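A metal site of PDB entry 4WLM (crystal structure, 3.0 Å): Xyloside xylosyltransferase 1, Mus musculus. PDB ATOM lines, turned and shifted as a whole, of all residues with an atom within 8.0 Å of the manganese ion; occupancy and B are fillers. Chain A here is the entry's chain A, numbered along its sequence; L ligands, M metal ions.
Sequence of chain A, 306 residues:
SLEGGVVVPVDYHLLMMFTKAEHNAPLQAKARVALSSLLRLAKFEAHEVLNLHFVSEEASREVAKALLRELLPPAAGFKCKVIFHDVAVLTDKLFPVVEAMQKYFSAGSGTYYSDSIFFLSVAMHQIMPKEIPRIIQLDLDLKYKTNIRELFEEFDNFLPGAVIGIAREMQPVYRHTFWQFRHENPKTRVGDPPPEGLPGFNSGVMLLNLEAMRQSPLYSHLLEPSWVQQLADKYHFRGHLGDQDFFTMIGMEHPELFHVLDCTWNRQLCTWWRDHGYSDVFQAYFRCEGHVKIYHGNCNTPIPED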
ATOM      1  N   LYS A  30      -5.329  -4.870  27.926  1.00  0.00           N
ATOM      2  CA  LYS A  30      -5.560  -5.453  26.603  1.00  0.00           C
ATOM      3  C   LYS A  30      -4.661  -6.654  26.359  1.00  0.00           C
ATOM      4  O   LYS A  30      -5.120  -7.706  25.914  1.00  0.00           O
ATOM      5  CB  LYS A  30      -5.326  -4.415  25.509  1.00  0.00           C
ATOM      6  CG  LYS A  30      -6.470  -3.433  25.295  1.00  0.00           C
ATOM      7  CD  LYS A  30      -6.097  -2.410  24.231  1.00  0.00           C
ATOM      8  CE  LYS A  30      -7.180  -1.358  24.064  1.00  0.00           C
ATOM      9  NZ  LYS A  30      -6.810  -0.352  23.026  1.00  0.00           N
ATOM     10  N   LEU A 138       0.131  -9.336  14.802  1.00  0.00           N
ATOM     11  CA  LEU A 138      -1.115  -9.313  15.547  1.00  0.00           C
ATOM     12  C   LEU A 138      -1.211  -8.107  16.476  1.00  0.00           C
ATOM     13  O   LEU A 138      -0.214  -7.675  17.057  1.00  0.00           O
ATOM     14  CB  LEU A 138      -1.276 -10.607  16.359  1.00  0.00           C
ATOM     15  CG  LEU A 138      -1.413 -11.930  15.605  1.00  0.00           C
ATOM     16  CD1 LEU A 138      -0.899 -13.091  16.455  1.00  0.00           C
ATOM     17  CD2 LEU A 138      -2.853 -12.185  15.169  1.00  0.00           C
ATOM     18  N   ASP A 139      -2.414  -7.564  16.602  1.00  0.00           N
ATOM     19  CA  ASP A 139      -2.716  -6.500  17.556  1.00  0.00           C
ATOM     20  C   ASP A 139      -2.790  -7.066  18.979  1.00  0.00           C
ATOM     21  O   ASP A 139      -2.751  -8.283  19.179  1.00  0.00           O
ATOM     22  CB  ASP A 139      -4.031  -5.810  17.192  1.00  0.00           C
ATOM     23  CG  ASP A 139      -3.868  -4.731  16.135  1.00  0.00           C
ATOM     24  OD1 ASP A 139      -2.789  -4.647  15.509  1.00  0.00           O
ATOM     25  OD2 ASP A 139      -4.822  -3.959  15.929  1.00  0.00           O
ATOM     26  N   LEU A 140      -2.900  -6.172  19.964  1.00  0.00           N
ATOM     27  CA  LEU A 140      -3.015  -6.585  21.358  1.00  0.00           C
ATOM     28  C   LEU A 140      -4.429  -6.363  21.915  1.00  0.00           C
ATOM     29  O   LEU A 140      -4.720  -6.742  23.049  1.00  0.00           O
ATOM     30  CB  LEU A 140      -1.984  -5.868  22.234  1.00  0.00           C
ATOM     31  CG  LEU A 140      -0.498  -6.017  21.909  1.00  0.00           C
ATOM     32  CD1 LEU A 140       0.274  -5.012  22.741  1.00  0.00           C
ATOM     33  CD2 LEU A 140       0.011  -7.439  22.167  1.00  0.00           C
ATOM     34  N   ASP A 141      -5.279  -5.741  21.112  1.00  0.00           N
ATOM     35  CA  ASP A 141      -6.691  -5.597  21.454  1.00  0.00           C
ATOM     36  C   ASP A 141      -7.507  -6.741  20.849  1.00  0.00           C
ATOM     37  O   ASP A 141      -8.663  -6.560  20.452  1.00  0.00           O
ATOM     38  CB  ASP A 141      -7.240  -4.210  21.058  1.00  0.00           C
ATOM     39  CG  ASP A 141      -6.868  -3.809  19.640  1.00  0.00           C
ATOM     40  OD1 ASP A 141      -5.797  -4.222  19.134  1.00  0.00           O
ATOM     41  OD2 ASP A 141      -7.642  -3.050  19.025  1.00  0.00           O
ATOM     42  N   LEU A 142      -6.885  -7.915  20.801  1.00  0.00           N
ATOM     43  CA  LEU A 142      -7.503  -9.122  20.260  1.00  0.00           C
ATOM     44  C   LEU A 142      -7.883 -10.101  21.367  1.00  0.00           C
ATOM     45  O   LEU A 142      -7.304 -10.077  22.452  1.00  0.00           O
ATOM     46  CB  LEU A 142      -6.557  -9.822  19.273  1.00  0.00           C
ATOM     47  CG  LEU A 142      -6.125  -9.105  17.984  1.00  0.00           C
ATOM     48  CD1 LEU A 142      -4.971  -9.851  17.337  1.00  0.00           C
ATOM     49  CD2 LEU A 142      -7.276  -8.964  17.008  1.00  0.00           C
ATOM     50  N   ASN A 202      -8.379  -4.431   7.352  1.00  0.00           N
ATOM     51  CA  ASN A 202      -8.035  -4.155   8.741  1.00  0.00           C
ATOM     52  C   ASN A 202      -6.717  -4.849   9.072  1.00  0.00           C
ATOM     53  O   ASN A 202      -6.562  -6.040   8.816  1.00  0.00           O
ATOM     54  CB  ASN A 202      -9.128  -4.655   9.682  1.00  0.00           C
ATOM     55  CG  ASN A 202      -8.883  -4.277  11.130  1.00  0.00           C
ATOM     56  OD1 ASN A 202      -9.115  -3.144  11.532  1.00  0.00           O
ATOM     57  ND2 ASN A 202      -8.404  -5.231  11.913  1.00  0.00           N
ATOM     58  N   SER A 203      -5.781  -4.088   9.637  1.00  0.00           N
ATOM     59  CA  SER A 203      -4.422  -4.571   9.869  1.00  0.00           C
ATOM     60  C   SER A 203      -4.224  -5.296  11.207  1.00  0.00           C
ATOM     61  O   SER A 203      -3.100  -5.646  11.568  1.00  0.00           O
ATOM     62  CB  SER A 203      -3.417  -3.417   9.731  1.00  0.00           C
ATOM     63  OG  SER A 203      -3.709  -2.375  10.649  1.00  0.00           O
ATOM     64  N   GLY A 204      -5.317  -5.534  11.924  1.00  0.00           N
ATOM     65  CA  GLY A 204      -5.283  -6.198  13.228  1.00  0.00           C
ATOM     66  C   GLY A 204      -4.686  -7.598  13.213  1.00  0.00           C
ATOM     67  O   GLY A 204      -3.944  -7.977  14.124  1.00  0.00           O
ATOM     68  N   VAL A 205      -5.020  -8.363  12.166  1.00  0.00           N
ATOM     69  CA  VAL A 205      -4.502  -9.718  11.984  1.00  0.00           C
ATOM     70  C   VAL A 205      -3.961  -9.838  10.552  1.00  0.00           C
ATOM     71  O   VAL A 205      -4.731  -9.755   9.590  1.00  0.00           O
ATOM     72  CB  VAL A 205      -5.579 -10.795  12.255  1.00  0.00           C
ATOM     73  CG1 VAL A 205      -5.033 -12.196  11.971  1.00  0.00           C
ATOM     74  CG2 VAL A 205      -6.087 -10.705  13.687  1.00  0.00           C
ATOM     75  N   GLN A 244      -2.068  -0.087   7.251  1.00  0.00           N
ATOM     76  CA  GLN A 244      -3.406  -0.483   6.852  1.00  0.00           C
ATOM     77  C   GLN A 244      -3.855   0.246   5.592  1.00  0.00           C
ATOM     78  O   GLN A 244      -4.446  -0.346   4.702  1.00  0.00           O
ATOM     79  CB  GLN A 244      -4.393  -0.225   7.999  1.00  0.00           C
ATOM     80  CG  GLN A 244      -5.754  -0.866   7.802  1.00  0.00           C
ATOM     81  CD  GLN A 244      -6.735  -0.522   8.911  1.00  0.00           C
ATOM     82  OE1 GLN A 244      -6.497  -0.826  10.082  1.00  0.00           O
ATOM     83  NE2 GLN A 244      -7.845   0.100   8.536  1.00  0.00           N
ATOM     84  N   ASN A 266     -11.070 -12.109  12.379  1.00  0.00           N
ATOM     85  CA  ASN A 266     -10.879 -10.767  12.863  1.00  0.00           C
ATOM     86  C   ASN A 266     -12.200 -10.041  12.927  1.00  0.00           C
ATOM     87  O   ASN A 266     -12.441  -9.146  12.153  1.00  0.00           O
ATOM     88  CB  ASN A 266      -9.924 -10.055  11.897  1.00  0.00           C
ATOM     89  CG  ASN A 266      -9.346  -8.793  12.465  1.00  0.00           C
ATOM     90  OD1 ASN A 266      -9.491  -8.503  13.618  1.00  0.00           O
ATOM     91  ND2 ASN A 266      -8.649  -8.071  11.652  1.00  0.00           N
ATOM     92  N   GLN A 268     -14.044  -7.370  14.083  1.00  0.00           N
ATOM     93  CA  GLN A 268     -13.805  -6.079  14.704  1.00  0.00           C
ATOM     94  C   GLN A 268     -15.097  -5.599  15.367  1.00  0.00           C
ATOM     95  O   GLN A 268     -16.167  -5.663  14.769  1.00  0.00           O
ATOM     96  CB  GLN A 268     -13.332  -5.075  13.659  1.00  0.00           C
ATOM     97  CG  GLN A 268     -12.059  -5.490  12.957  1.00  0.00           C
ATOM     98  CD  GLN A 268     -12.095  -5.217  11.463  1.00  0.00           C
ATOM     99  OE1 GLN A 268     -12.025  -6.139  10.653  1.00  0.00           O
ATOM    100  NE2 GLN A 268     -12.210  -3.935  11.102  1.00  0.00           N
ATOM    101  N   HIS A 296     -11.576  -8.742  17.559  1.00  0.00           N
ATOM    102  CA  HIS A 296     -10.720  -7.564  17.605  1.00  0.00           C
ATOM    103  C   HIS A 296     -11.525  -6.447  18.202  1.00  0.00           C
ATOM    104  O   HIS A 296     -12.408  -5.890  17.554  1.00  0.00           O
ATOM    105  CB  HIS A 296     -10.218  -7.182  16.213  1.00  0.00           C
ATOM    106  CG  HIS A 296      -9.188  -6.064  16.199  1.00  0.00           C
ATOM    107  ND1 HIS A 296      -8.800  -5.468  15.056  1.00  0.00           N
ATOM    108  CD2 HIS A 296      -8.486  -5.453  17.230  1.00  0.00           C
ATOM    109  CE1 HIS A 296      -7.884  -4.519  15.340  1.00  0.00           C
ATOM    110  NE2 HIS A 296      -7.697  -4.502  16.667  1.00  0.00           N
ATOM    111  N   GLY A 297     -11.232  -6.144  19.457  1.00  0.00           N
ATOM    112  CA  GLY A 297     -11.896  -5.042  20.139  1.00  0.00           C
ATOM    113  C   GLY A 297     -11.231  -3.741  19.723  1.00  0.00           C
ATOM    114  O   GLY A 297     -10.659  -3.051  20.572  1.00  0.00           O
ATOM    115  N   ASN A 298     -11.303  -3.414  18.439  1.00  0.00           N
ATOM    116  CA  ASN A 298     -10.706  -2.166  17.980  1.00  0.00           C
ATOM    117  C   ASN A 298     -11.462  -0.943  18.524  1.00  0.00           C
ATOM    118  O   ASN A 298     -12.624  -1.039  18.922  1.00  0.00           O
ATOM    119  CB  ASN A 298     -10.477  -2.120  16.453  1.00  0.00           C
ATOM    120  CG  ASN A 298     -11.758  -2.260  15.641  1.00  0.00           C
ATOM    121  OD1 ASN A 298     -12.738  -2.851  16.090  1.00  0.00           O
ATOM    122  ND2 ASN A 298     -11.735  -1.721  14.422  1.00  0.00           N
ATOM    123  N   CYS A 299     -10.742   0.182  18.563  1.00  0.00           N
ATOM    124  CA  CYS A 299     -11.190   1.437  19.183  1.00  0.00           C
ATOM    125  C   CYS A 299     -11.703   1.292  20.630  1.00  0.00           C
ATOM    126  O   CYS A 299     -12.741   1.855  20.995  1.00  0.00           O
ATOM    127  CB  CYS A 299     -12.173   2.203  18.271  1.00  0.00           C
ATOM    128  SG  CYS A 299     -13.930   1.739  18.369  1.00  0.00           S
ATOM    129  N   ASN A 300     -10.951   0.551  21.448  1.00  0.00           N
ATOM    130  CA  ASN A 300     -11.224   0.394  22.888  1.00  0.00           C
ATOM    131  C   ASN A 300     -12.563  -0.271  23.257  1.00  0.00           C
ATOM    132  O   ASN A 300     -13.048  -0.123  24.379  1.00  0.00           O
ATOM    133  CB  ASN A 300     -11.079   1.732  23.638  1.00  0.00           C
ATOM    134  CG  ASN A 300      -9.670   2.273  23.603  1.00  0.00           C
ATOM    135  OD1 ASN A 300      -8.732   1.647  24.095  1.00  0.00           O
ATOM    136  ND2 ASN A 300      -9.507   3.465  23.040  1.00  0.00           N
HETATM  137  S1  LIG L   1      -7.478   0.573  16.699  1.00  0.00           S
HETATM  138  O1  LIG L   1      -7.697   0.506  18.125  1.00  0.00           O
HETATM  139  O2  LIG L   1      -8.635   1.145  16.029  1.00  0.00           O
HETATM  140  O3  LIG L   1      -7.131  -0.768  16.200  1.00  0.00           O
HETATM  141  O4  LIG L   1      -6.297   1.386  16.483  1.00  0.00           O
HETATM  142 MN    MN M   1      -6.435  -3.144  17.028  1.00  0.00          MN
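The backbone carbonyl oxygen (O) of His 296 sits close to the side-chain amide oxygen (OD1) of Asn 298 (3.4 Å). ND2 of Asn 202 is in hydrogen-bond range of ND1 of His 296, 3.2 Å away. OD1 of Asn 266 sits close to ND1 of His 296, at 3.4 Å. O of Gly 204 lies within hydrogen-bond range of N of Asp 139 (2.9 Å). The backbone carbonyl oxygen (O) of Asp 141 lies within hydrogen-bond range of the backbone NH (N) of Gly 297 (2.8 Å).
The manganese ion is bound by NE2 of His 296, OD2 of Asp 139, OD2 of Asp 141, OD1 of Asp 141 and O3 of the ligand. The manganese ion has five donor atoms within binding distance.
Of the 18 residues printed, 3 come within 4 Å of the manganese ion.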
